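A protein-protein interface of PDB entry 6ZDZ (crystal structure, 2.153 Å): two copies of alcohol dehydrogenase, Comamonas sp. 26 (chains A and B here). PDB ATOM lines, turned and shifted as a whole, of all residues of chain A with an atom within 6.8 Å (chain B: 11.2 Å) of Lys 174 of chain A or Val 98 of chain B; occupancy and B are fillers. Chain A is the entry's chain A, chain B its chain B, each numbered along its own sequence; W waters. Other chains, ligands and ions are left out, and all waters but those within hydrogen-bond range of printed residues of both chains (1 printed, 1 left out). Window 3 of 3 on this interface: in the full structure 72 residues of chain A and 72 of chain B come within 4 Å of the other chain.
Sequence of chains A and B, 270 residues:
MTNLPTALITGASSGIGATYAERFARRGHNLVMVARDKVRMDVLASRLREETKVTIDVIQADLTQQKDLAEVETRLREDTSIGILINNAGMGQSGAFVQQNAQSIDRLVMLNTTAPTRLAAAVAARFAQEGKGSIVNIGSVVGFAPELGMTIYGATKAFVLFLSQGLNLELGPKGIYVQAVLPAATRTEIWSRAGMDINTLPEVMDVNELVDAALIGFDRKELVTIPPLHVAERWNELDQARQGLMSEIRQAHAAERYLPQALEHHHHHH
Water W1 lies within hydrogen-bond range of OE1 of Glu 170 of chain A (2.5 Å), N of Val 98 of chain B (3.2 Å) and N of Phe 97 of chain B (3.3 Å).
N of Ala 96 of chain B sits at hydrogen-bond distance from OE1 of Gln 99 of chain B (3.4 Å).
The backbone carbonyl oxygen of Ala 96 of chain B sits at hydrogen-bond distance from the side-chain amide nitrogen of Gln 100 of chain B (3.1 Å).
No position is printed for both chains.
OE1 of Glu 170 of chain A lies within hydrogen-bond range of N of Phe 97 of chain B (2.6 Å).
OG1 of Thr 151 of chain B lies within hydrogen-bond range of OE2 of Glu 170 of chain A (2.8 Å).
Printed residues of chain A that touch a printed residue of chain B: Ala 121, Ala 124, Glu 170 and Lys 174.
Hydrophobic or aromatic side chains of chain A that line the printed part of chain B: Ala 121 and Ala 124.
Along chain B the printed residues that touch a printed residue of chain A span positions 96 to 151.
Among the printed residues, 7 pairs touch across the chains.
Ala 124 of chain A touches one residue of chain B.
Ala 125 of chain A touches none of the printed residues of chain B.
Glu 130 of chain A touches none of the printed residues of chain B.
No residue of chain B comes within 4 Å of Gly 131 of chain A.
Of the printed residues of chain B, Glu 170 of chain A touches Ala 96 (3.4 Å), Phe 97 (2.6 Å) and Thr 151 (2.8 Å).
No residue of chain B comes within 4 Å of Leu 171 of chain A.
No residue of chain B comes within 4 Å of Gly 172 of chain A.
Lys 174 of chain A touches just one residue of chain B: Val 98 (3.7 Å).
No residue of chain B comes within 4 Å of Gly 175 of chain A.
No residue of chain B comes within 4 Å of Ile 176 of chain A.
Of the printed residues of chain A, Ala 96 of chain B touches Glu 170 (3.4 Å).
Of the printed residues of chain A, Phe 97 of chain B touches Ala 121, Ala 124 and Glu 170.
Of chain A, only Lys 174 comes within 4 Å of Val 98 of chain B.
Of the printed residues of chain A, Ile 105 of chain B touches Ala 121 (3.8 Å).
Met 150 of chain B touches none of the printed residues of chain A.
Printed residues of chain A within 4 Å of Thr 151 of chain B: Glu 170 (2.8 Å).
The nearest residue of chain A that does not touch Val 98 of chain B is Leu 171 of chain A (4.1 Å).
The nearest printed residue of chain A that does not touch Thr 151 of chain B is Asn 168 of chain A (6.5 Å).
Among the printed residues, merely in contact across the chains: Ala 121 of chain A with Phe 97 of chain B, Ala 121 of chain A with Ile 105 of chain B, Ala 124 of chain A with Phe 97 of chain B, Glu 170 of chain A with Ala 96 of chain B and Lys 174 of chain A with Val 98 of chain B.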
ATOM      1  N   ALA A 121      15.553  -0.380   8.839  1.00  0.00           N
ATOM      2  CA  ALA A 121      14.885  -1.272   7.898  1.00  0.00           C
ATOM      3  C   ALA A 121      13.471  -0.803   7.581  1.00  0.00           C
ATOM      4  O   ALA A 121      12.964  -1.065   6.485  1.00  0.00           O
ATOM      5  CB  ALA A 121      14.861  -2.698   8.450  1.00  0.00           C
ATOM      6  N   ALA A 124      14.105   2.042   5.030  1.00  0.00           N
ATOM      7  CA  ALA A 124      14.994   1.756   3.908  1.00  0.00           C
ATOM      8  C   ALA A 124      14.208   1.508   2.628  1.00  0.00           C
ATOM      9  O   ALA A 124      14.543   2.047   1.565  1.00  0.00           O
ATOM     10  CB  ALA A 124      15.882   0.555   4.237  1.00  0.00           C
ATOM     11  N   ALA A 125      13.155   0.690   2.708  1.00  0.00           N
ATOM     12  CA  ALA A 125      12.388   0.355   1.512  1.00  0.00           C
ATOM     13  C   ALA A 125      11.684   1.582   0.944  1.00  0.00           C
ATOM     14  O   ALA A 125      11.662   1.784  -0.276  1.00  0.00           O
ATOM     15  CB  ALA A 125      11.377  -0.745   1.828  1.00  0.00           C
ATOM     16  N   PHE A 127      12.565   4.783   1.483  1.00  0.00           N
ATOM     17  CA  PHE A 127      13.587   5.713   1.009  1.00  0.00           C
ATOM     18  C   PHE A 127      14.124   5.304  -0.356  1.00  0.00           C
ATOM     19  O   PHE A 127      14.449   6.168  -1.179  1.00  0.00           O
ATOM     20  CB  PHE A 127      14.734   5.806   2.017  1.00  0.00           C
ATOM     21  CG  PHE A 127      14.434   6.669   3.213  1.00  0.00           C
ATOM     22  CD1 PHE A 127      13.194   7.267   3.368  1.00  0.00           C
ATOM     23  CD2 PHE A 127      15.401   6.886   4.182  1.00  0.00           C
ATOM     24  CE1 PHE A 127      12.924   8.062   4.466  1.00  0.00           C
ATOM     25  CE2 PHE A 127      15.136   7.679   5.283  1.00  0.00           C
ATOM     26  CZ  PHE A 127      13.896   8.268   5.425  1.00  0.00           C
ATOM     27  N   ALA A 128      14.229   3.997  -0.614  1.00  0.00           N
ATOM     28  CA  ALA A 128      14.689   3.535  -1.919  1.00  0.00           C
ATOM     29  C   ALA A 128      13.654   3.815  -3.002  1.00  0.00           C
ATOM     30  O   ALA A 128      14.011   4.150  -4.137  1.00  0.00           O
ATOM     31  CB  ALA A 128      15.020   2.045  -1.860  1.00  0.00           C
ATOM     32  N   GLN A 129      12.368   3.666  -2.674  1.00  0.00           N
ATOM     33  CA  GLN A 129      11.309   4.043  -3.607  1.00  0.00           C
ATOM     34  C   GLN A 129      11.418   5.510  -4.004  1.00  0.00           C
ATOM     35  O   GLN A 129      11.466   5.843  -5.193  1.00  0.00           O
ATOM     36  CB  GLN A 129       9.939   3.754  -2.992  1.00  0.00           C
ATOM     37  CG  GLN A 129       9.512   2.301  -3.068  1.00  0.00           C
ATOM     38  CD  GLN A 129       9.017   1.921  -4.450  1.00  0.00           C
ATOM     39  OE1 GLN A 129       8.802   2.782  -5.305  1.00  0.00           O
ATOM     40  NE2 GLN A 129       8.830   0.625  -4.677  1.00  0.00           N
ATOM     41  N   GLU A 130      11.462   6.403  -3.015  1.00  0.00           N
ATOM     42  CA  GLU A 130      11.493   7.834  -3.288  1.00  0.00           C
ATOM     43  C   GLU A 130      12.840   8.306  -3.818  1.00  0.00           C
ATOM     44  O   GLU A 130      12.922   9.425  -4.336  1.00  0.00           O
ATOM     45  CB  GLU A 130      11.141   8.608  -2.017  1.00  0.00           C
ATOM     46  CG  GLU A 130       9.866   8.130  -1.339  1.00  0.00           C
ATOM     47  CD  GLU A 130       9.618   8.815  -0.010  1.00  0.00           C
ATOM     48  OE1 GLU A 130       8.659   8.427   0.690  1.00  0.00           O
ATOM     49  OE2 GLU A 130      10.385   9.738   0.339  1.00  0.00           O
ATOM     50  N   GLY A 131      13.888   7.490  -3.709  1.00  0.00           N
ATOM     51  CA  GLY A 131      15.202   7.912  -4.149  1.00  0.00           C
ATOM     52  C   GLY A 131      15.836   8.981  -3.292  1.00  0.00           C
ATOM     53  O   GLY A 131      16.725   9.695  -3.764  1.00  0.00           O
ATOM     54  N   LYS A 132      15.406   9.112  -2.040  1.00  0.00           N
ATOM     55  CA  LYS A 132      15.920  10.142  -1.151  1.00  0.00           C
ATOM     56  C   LYS A 132      15.673   9.708   0.286  1.00  0.00           C
ATOM     57  O   LYS A 132      14.941   8.752   0.551  1.00  0.00           O
ATOM     58  CB  LYS A 132      15.266  11.501  -1.424  1.00  0.00           C
ATOM     59  CG  LYS A 132      13.747  11.483  -1.326  1.00  0.00           C
ATOM     60  CD  LYS A 132      13.144  12.831  -1.682  1.00  0.00           C
ATOM     61  CE  LYS A 132      11.637  12.830  -1.478  1.00  0.00           C
ATOM     62  NZ  LYS A 132      11.046  14.178  -1.698  1.00  0.00           N
ATOM     63  N   GLY A 133      16.296  10.429   1.214  1.00  0.00           N
ATOM     64  CA  GLY A 133      16.159  10.129   2.624  1.00  0.00           C
ATOM     65  C   GLY A 133      17.481  10.139   3.363  1.00  0.00           C
ATOM     66  O   GLY A 133      18.545  10.003   2.751  1.00  0.00           O
ATOM     67  N   ASN A 168      25.487   2.716   4.104  1.00  0.00           N
ATOM     68  CA  ASN A 168      25.932   3.692   3.116  1.00  0.00           C
ATOM     69  C   ASN A 168      26.222   3.028   1.776  1.00  0.00           C
ATOM     70  O   ASN A 168      25.756   3.487   0.728  1.00  0.00           O
ATOM     71  CB  ASN A 168      27.166   4.433   3.628  1.00  0.00           C
ATOM     72  CG  ASN A 168      27.840   5.251   2.545  1.00  0.00           C
ATOM     73  OD1 ASN A 168      27.363   6.321   2.172  1.00  0.00           O
ATOM     74  ND2 ASN A 168      28.957   4.747   2.033  1.00  0.00           N
ATOM     75  N   GLU A 170      25.129   0.268   0.666  1.00  0.00           N
ATOM     76  CA  GLU A 170      23.945  -0.385   0.124  1.00  0.00           C
ATOM     77  C   GLU A 170      22.885   0.617  -0.317  1.00  0.00           C
ATOM     78  O   GLU A 170      22.252   0.430  -1.361  1.00  0.00           O
ATOM     79  CB  GLU A 170      23.353  -1.345   1.159  1.00  0.00           C
ATOM     80  CG  GLU A 170      23.244  -2.782   0.681  1.00  0.00           C
ATOM     81  CD  GLU A 170      22.728  -3.719   1.757  1.00  0.00           C
ATOM     82  OE1 GLU A 170      21.744  -4.443   1.496  1.00  0.00           O
ATOM     83  OE2 GLU A 170      23.296  -3.722   2.871  1.00  0.00           O
ATOM     84  N   LEU A 171      22.679   1.680   0.461  1.00  0.00           N
ATOM     85  CA  LEU A 171      21.615   2.639   0.197  1.00  0.00           C
ATOM     86  C   LEU A 171      22.101   3.915  -0.476  1.00  0.00           C
ATOM     87  O   LEU A 171      21.281   4.637  -1.055  1.00  0.00           O
ATOM     88  CB  LEU A 171      20.897   2.999   1.503  1.00  0.00           C
ATOM     89  CG  LEU A 171      20.335   1.816   2.293  1.00  0.00           C
ATOM     90  CD1 LEU A 171      19.784   2.270   3.633  1.00  0.00           C
ATOM     91  CD2 LEU A 171      19.267   1.092   1.488  1.00  0.00           C
ATOM     92  N   GLY A 172      23.398   4.210  -0.403  1.00  0.00           N
ATOM     93  CA  GLY A 172      23.972   5.376  -1.037  1.00  0.00           C
ATOM     94  C   GLY A 172      23.667   5.485  -2.520  1.00  0.00           C
ATOM     95  O   GLY A 172      23.167   6.511  -2.991  1.00  0.00           O
ATOM     96  N   PRO A 173      23.970   4.434  -3.289  1.00  0.00           N
ATOM     97  CA  PRO A 173      23.639   4.456  -4.725  1.00  0.00           C
ATOM     98  C   PRO A 173      22.158   4.641  -5.013  1.00  0.00           C
ATOM     99  O   PRO A 173      21.802   4.948  -6.158  1.00  0.00           O
ATOM    100  CB  PRO A 173      24.132   3.091  -5.222  1.00  0.00           C
ATOM    101  CG  PRO A 173      25.219   2.726  -4.279  1.00  0.00           C
ATOM    102  CD  PRO A 173      24.800   3.266  -2.940  1.00  0.00           C
ATOM    103  N   LYS A 174      21.288   4.464  -4.020  1.00  0.00           N
ATOM    104  CA  LYS A 174      19.856   4.660  -4.179  1.00  0.00           C
ATOM    105  C   LYS A 174      19.411   6.065  -3.795  1.00  0.00           C
ATOM    106  O   LYS A 174      18.207   6.341  -3.784  1.00  0.00           O
ATOM    107  CB  LYS A 174      19.104   3.630  -3.335  1.00  0.00           C
ATOM    108  CG  LYS A 174      19.279   2.201  -3.816  1.00  0.00           C
ATOM    109  CD  LYS A 174      18.663   1.211  -2.843  1.00  0.00           C
ATOM    110  CE  LYS A 174      18.810  -0.218  -3.341  1.00  0.00           C
ATOM    111  NZ  LYS A 174      18.286  -1.205  -2.357  1.00  0.00           N
ATOM    112  N   GLY A 175      20.352   6.956  -3.487  1.00  0.00           N
ATOM    113  CA  GLY A 175      20.031   8.319  -3.124  1.00  0.00           C
ATOM    114  C   GLY A 175      19.855   8.563  -1.643  1.00  0.00           C
ATOM    115  O   GLY A 175      19.372   9.637  -1.264  1.00  0.00           O
ATOM    116  N   ILE A 176      20.231   7.609  -0.796  1.00  0.00           N
ATOM    117  CA  ILE A 176      20.021   7.696   0.644  1.00  0.00           C
ATOM    118  C   ILE A 176      21.324   8.105   1.314  1.00  0.00           C
ATOM    119  O   ILE A 176      22.390   7.554   1.008  1.00  0.00           O
ATOM    120  CB  ILE A 176      19.506   6.360   1.206  1.00  0.00           C
ATOM    121  CG1 ILE A 176      18.176   5.986   0.545  1.00  0.00           C
ATOM    122  CG2 ILE A 176      19.355   6.435   2.718  1.00  0.00           C
ATOM    123  CD1 ILE A 176      17.803   4.529   0.697  1.00  0.00           C
ATOM    124  N   GLN B  93      23.176 -13.942   7.273  1.00  0.00           N
ATOM    125  CA  GLN B  93      22.174 -13.022   6.751  1.00  0.00           C
ATOM    126  C   GLN B  93      21.719 -13.459   5.364  1.00  0.00           C
ATOM    127  O   GLN B  93      22.526 -13.911   4.547  1.00  0.00           O
ATOM    128  CB  GLN B  93      22.720 -11.594   6.693  1.00  0.00           C
ATOM    129  CG  GLN B  93      21.659 -10.538   6.424  1.00  0.00           C
ATOM    130  CD  GLN B  93      22.194  -9.125   6.555  1.00  0.00           C
ATOM    131  OE1 GLN B  93      23.268  -8.906   7.115  1.00  0.00           O
ATOM    132  NE2 GLN B  93      21.446  -8.158   6.034  1.00  0.00           N
ATOM    133  N   SER B  94      20.419 -13.319   5.107  1.00  0.00           N
ATOM    134  CA  SER B  94      19.822 -13.729   3.836  1.00  0.00           C
ATOM    135  C   SER B  94      19.746 -12.522   2.908  1.00  0.00           C
ATOM    136  O   SER B  94      18.753 -11.794   2.877  1.00  0.00           O
ATOM    137  CB  SER B  94      18.447 -14.348   4.063  1.00  0.00           C
ATOM    138  OG  SER B  94      17.933 -14.897   2.862  1.00  0.00           O
ATOM    139  N   GLY B  95      20.811 -12.309   2.141  1.00  0.00           N
ATOM    140  CA  GLY B  95      20.807 -11.318   1.080  1.00  0.00           C
ATOM    141  C   GLY B  95      20.977  -9.875   1.513  1.00  0.00           C
ATOM    142  O   GLY B  95      21.808  -9.567   2.374  1.00  0.00           O
ATOM    143  N   ALA B  96      20.187  -8.982   0.921  1.00  0.00           N
ATOM    144  CA  ALA B  96      20.363  -7.548   1.085  1.00  0.00           C
ATOM    145  C   ALA B  96      19.598  -7.026   2.300  1.00  0.00           C
ATOM    146  O   ALA B  96      18.794  -7.728   2.918  1.00  0.00           O
ATOM    147  CB  ALA B  96      19.918  -6.807  -0.176  1.00  0.00           C
ATOM    148  N   PHE B  97      19.860  -5.758   2.631  1.00  0.00           N
ATOM    149  CA  PHE B  97      19.271  -5.159   3.824  1.00  0.00           C
ATOM    150  C   PHE B  97      17.795  -4.838   3.623  1.00  0.00           C
ATOM    151  O   PHE B  97      16.989  -5.005   4.546  1.00  0.00           O
ATOM    152  CB  PHE B  97      20.046  -3.900   4.212  1.00  0.00           C
ATOM    153  CG  PHE B  97      19.502  -3.202   5.425  1.00  0.00           C
ATOM    154  CD1 PHE B  97      19.850  -3.624   6.697  1.00  0.00           C
ATOM    155  CD2 PHE B  97      18.645  -2.120   5.295  1.00  0.00           C
ATOM    156  CE1 PHE B  97      19.352  -2.984   7.816  1.00  0.00           C
ATOM    157  CE2 PHE B  97      18.145  -1.475   6.410  1.00  0.00           C
ATOM    158  CZ  PHE B  97      18.500  -1.908   7.672  1.00  0.00           C
ATOM    159  N   VAL B  98      17.422  -4.364   2.431  1.00  0.00           N
ATOM    160  CA  VAL B  98      16.027  -4.025   2.174  1.00  0.00           C
ATOM    161  C   VAL B  98      15.131  -5.255   2.200  1.00  0.00           C
ATOM    162  O   VAL B  98      13.907  -5.123   2.316  1.00  0.00           O
ATOM    163  CB  VAL B  98      15.890  -3.290   0.828  1.00  0.00           C
ATOM    164  CG1 VAL B  98      16.644  -1.969   0.866  1.00  0.00           C
ATOM    165  CG2 VAL B  98      16.398  -4.165  -0.307  1.00  0.00           C
ATOM    166  N   GLN B  99      15.709  -6.449   2.097  1.00  0.00           N
ATOM    167  CA  GLN B  99      14.953  -7.691   2.168  1.00  0.00           C
ATOM    168  C   GLN B  99      14.834  -8.237   3.584  1.00  0.00           C
ATOM    169  O   GLN B  99      14.139  -9.237   3.789  1.00  0.00           O
ATOM    170  CB  GLN B  99      15.593  -8.744   1.258  1.00  0.00           C
ATOM    171  CG  GLN B  99      15.466  -8.424  -0.221  1.00  0.00           C
ATOM    172  CD  GLN B  99      16.201  -9.414  -1.101  1.00  0.00           C
ATOM    173  OE1 GLN B  99      17.350  -9.770  -0.831  1.00  0.00           O
ATOM    174  NE2 GLN B  99      15.543  -9.862  -2.164  1.00  0.00           N
ATOM    175  N   GLN B 100      15.494  -7.615   4.557  1.00  0.00           N
ATOM    176  CA  GLN B 100      15.401  -8.055   5.941  1.00  0.00           C
ATOM    177  C   GLN B 100      14.089  -7.589   6.557  1.00  0.00           C
ATOM    178  O   GLN B 100      13.652  -6.456   6.338  1.00  0.00           O
ATOM    179  CB  GLN B 100      16.574  -7.512   6.758  1.00  0.00           C
ATOM    180  CG  GLN B 100      17.946  -7.894   6.228  1.00  0.00           C
ATOM    181  CD  GLN B 100      18.161  -9.392   6.198  1.00  0.00           C
ATOM    182  OE1 GLN B 100      17.911 -10.087   7.184  1.00  0.00           O
ATOM    183  NE2 GLN B 100      18.629  -9.899   5.063  1.00  0.00           N
ATOM    184  N   ASN B 101      13.463  -8.469   7.329  1.00  0.00           N
ATOM    185  CA  ASN B 101      12.287  -8.116   8.106  1.00  0.00           C
ATOM    186  C   ASN B 101      12.651  -8.053   9.583  1.00  0.00           C
ATOM    187  O   ASN B 101      13.728  -8.485  10.001  1.00  0.00           O
ATOM    188  CB  ASN B 101      11.142  -9.111   7.857  1.00  0.00           C
ATOM    189  CG  ASN B 101      11.530 -10.554   8.150  1.00  0.00           C
ATOM    190  OD1 ASN B 101      12.290 -10.838   9.075  1.00  0.00           O
ATOM    191  ND2 ASN B 101      10.998 -11.476   7.356  1.00  0.00           N
ATOM    192  N   ALA B 102      11.734  -7.488  10.373  1.00  0.00           N
ATOM    193  CA  ALA B 102      11.991  -7.301  11.798  1.00  0.00           C
ATOM    194  C   ALA B 102      12.321  -8.621  12.483  1.00  0.00           C
ATOM    195  O   ALA B 102      13.165  -8.667  13.387  1.00  0.00           O
ATOM    196  CB  ALA B 102      10.788  -6.634  12.464  1.00  0.00           C
ATOM    197  N   GLN B 103      11.665  -9.706  12.067  1.00  0.00           N
ATOM    198  CA  GLN B 103      11.854 -10.990  12.734  1.00  0.00           C
ATOM    199  C   GLN B 103      13.233 -11.573  12.448  1.00  0.00           C
ATOM    200  O   GLN B 103      13.884 -12.113  13.351  1.00  0.00           O
ATOM    201  CB  GLN B 103      10.756 -11.963  12.303  1.00  0.00           C
ATOM    202  CG  GLN B 103      10.746 -13.276  13.060  1.00  0.00           C
ATOM    203  CD  GLN B 103       9.582 -14.161  12.659  1.00  0.00           C
ATOM    204  OE1 GLN B 103       8.707 -14.463  13.473  1.00  0.00           O
ATOM    205  NE2 GLN B 103       9.566 -14.582  11.399  1.00  0.00           N
ATOM    206  N   SER B 104      13.697 -11.478  11.198  1.00  0.00           N
ATOM    207  CA  SER B 104      15.026 -11.983  10.869  1.00  0.00           C
ATOM    208  C   SER B 104      16.120 -11.139  11.510  1.00  0.00           C
ATOM    209  O   SER B 104      17.185 -11.665  11.853  1.00  0.00           O
ATOM    210  CB  SER B 104      15.215 -12.035   9.354  1.00  0.00           C
ATOM    211  OG  SER B 104      15.264 -10.731   8.802  1.00  0.00           O
ATOM    212  N   ILE B 105      15.881  -9.838  11.672  1.00  0.00           N
ATOM    213  CA  ILE B 105      16.836  -8.989  12.377  1.00  0.00           C
ATOM    214  C   ILE B 105      16.909  -9.378  13.847  1.00  0.00           C
ATOM    215  O   ILE B 105      17.998  -9.471  14.426  1.00  0.00           O
ATOM    216  CB  ILE B 105      16.464  -7.506  12.197  1.00  0.00           C
ATOM    217  CG1 ILE B 105      16.564  -7.111  10.722  1.00  0.00           C
ATOM    218  CG2 ILE B 105      17.364  -6.619  13.046  1.00  0.00           C
ATOM    219  CD1 ILE B 105      15.954  -5.766  10.411  1.00  0.00           C
ATOM    220  N   LEU B 108      18.856 -12.661  14.050  1.00  0.00           N
ATOM    221  CA  LEU B 108      20.260 -12.501  13.688  1.00  0.00           C
ATOM    222  C   LEU B 108      21.042 -11.835  14.815  1.00  0.00           C
ATOM    223  O   LEU B 108      22.143 -12.274  15.166  1.00  0.00           O
ATOM    224  CB  LEU B 108      20.373 -11.697  12.391  1.00  0.00           C
ATOM    225  CG  LEU B 108      21.736 -11.580  11.708  1.00  0.00           C
ATOM    226  CD1 LEU B 108      22.456 -12.914  11.700  1.00  0.00           C
ATOM    227  CD2 LEU B 108      21.561 -11.062  10.291  1.00  0.00           C
ATOM    228  N   GLY B 149      28.489  -6.361   1.653  1.00  0.00           N
ATOM    229  CA  GLY B 149      27.043  -6.317   1.563  1.00  0.00           C
ATOM    230  C   GLY B 149      26.301  -7.140   2.588  1.00  0.00           C
ATOM    231  O   GLY B 149      25.082  -7.302   2.463  1.00  0.00           O
ATOM    232  N   MET B 150      26.989  -7.667   3.595  1.00  0.00           N
ATOM    233  CA  MET B 150      26.353  -8.370   4.704  1.00  0.00           C
ATOM    234  C   MET B 150      26.378  -7.462   5.931  1.00  0.00           C
ATOM    235  O   MET B 150      27.137  -7.668   6.883  1.00  0.00           O
ATOM    236  CB  MET B 150      27.054  -9.712   4.958  1.00  0.00           C
ATOM    237  CG  MET B 150      26.926 -10.694   3.796  1.00  0.00           C
ATOM    238  SD  MET B 150      27.927 -12.186   3.979  1.00  0.00           S
ATOM    239  CE  MET B 150      29.568 -11.544   3.652  1.00  0.00           C
ATOM    240  N   THR B 151      25.527  -6.435   5.889  1.00  0.00           N
ATOM    241  CA  THR B 151      25.626  -5.323   6.831  1.00  0.00           C
ATOM    242  C   THR B 151      25.328  -5.765   8.260  1.00  0.00           C
ATOM    243  O   THR B 151      26.143  -5.562   9.168  1.00  0.00           O
ATOM    244  CB  THR B 151      24.680  -4.199   6.407  1.00  0.00           C
ATOM    245  OG1 THR B 151      25.051  -3.724   5.108  1.00  0.00           O
ATOM    246  CG2 THR B 151      24.743  -3.050   7.399  1.00  0.00           C
ATOM    247  N   ILE B 152      24.159  -6.371   8.482  1.00  0.00           N
ATOM    248  CA  ILE B 152      23.771  -6.746   9.839  1.00  0.00           C
ATOM    249  C   ILE B 152      24.687  -7.839  10.374  1.00  0.00           C
ATOM    250  O   ILE B 152      25.162  -7.767  11.513  1.00  0.00           O
ATOM    251  CB  ILE B 152      22.295  -7.182   9.882  1.00  0.00           C
ATOM    252  CG1 ILE B 152      21.387  -6.061   9.378  1.00  0.00           C
ATOM    253  CG2 ILE B 152      21.902  -7.579  11.299  1.00  0.00           C
ATOM    254  CD1 ILE B 152      19.926  -6.445   9.324  1.00  0.00           C
HETATM  255  O   HOH W   1      19.817  -3.110   0.648  1.00  0.00           O
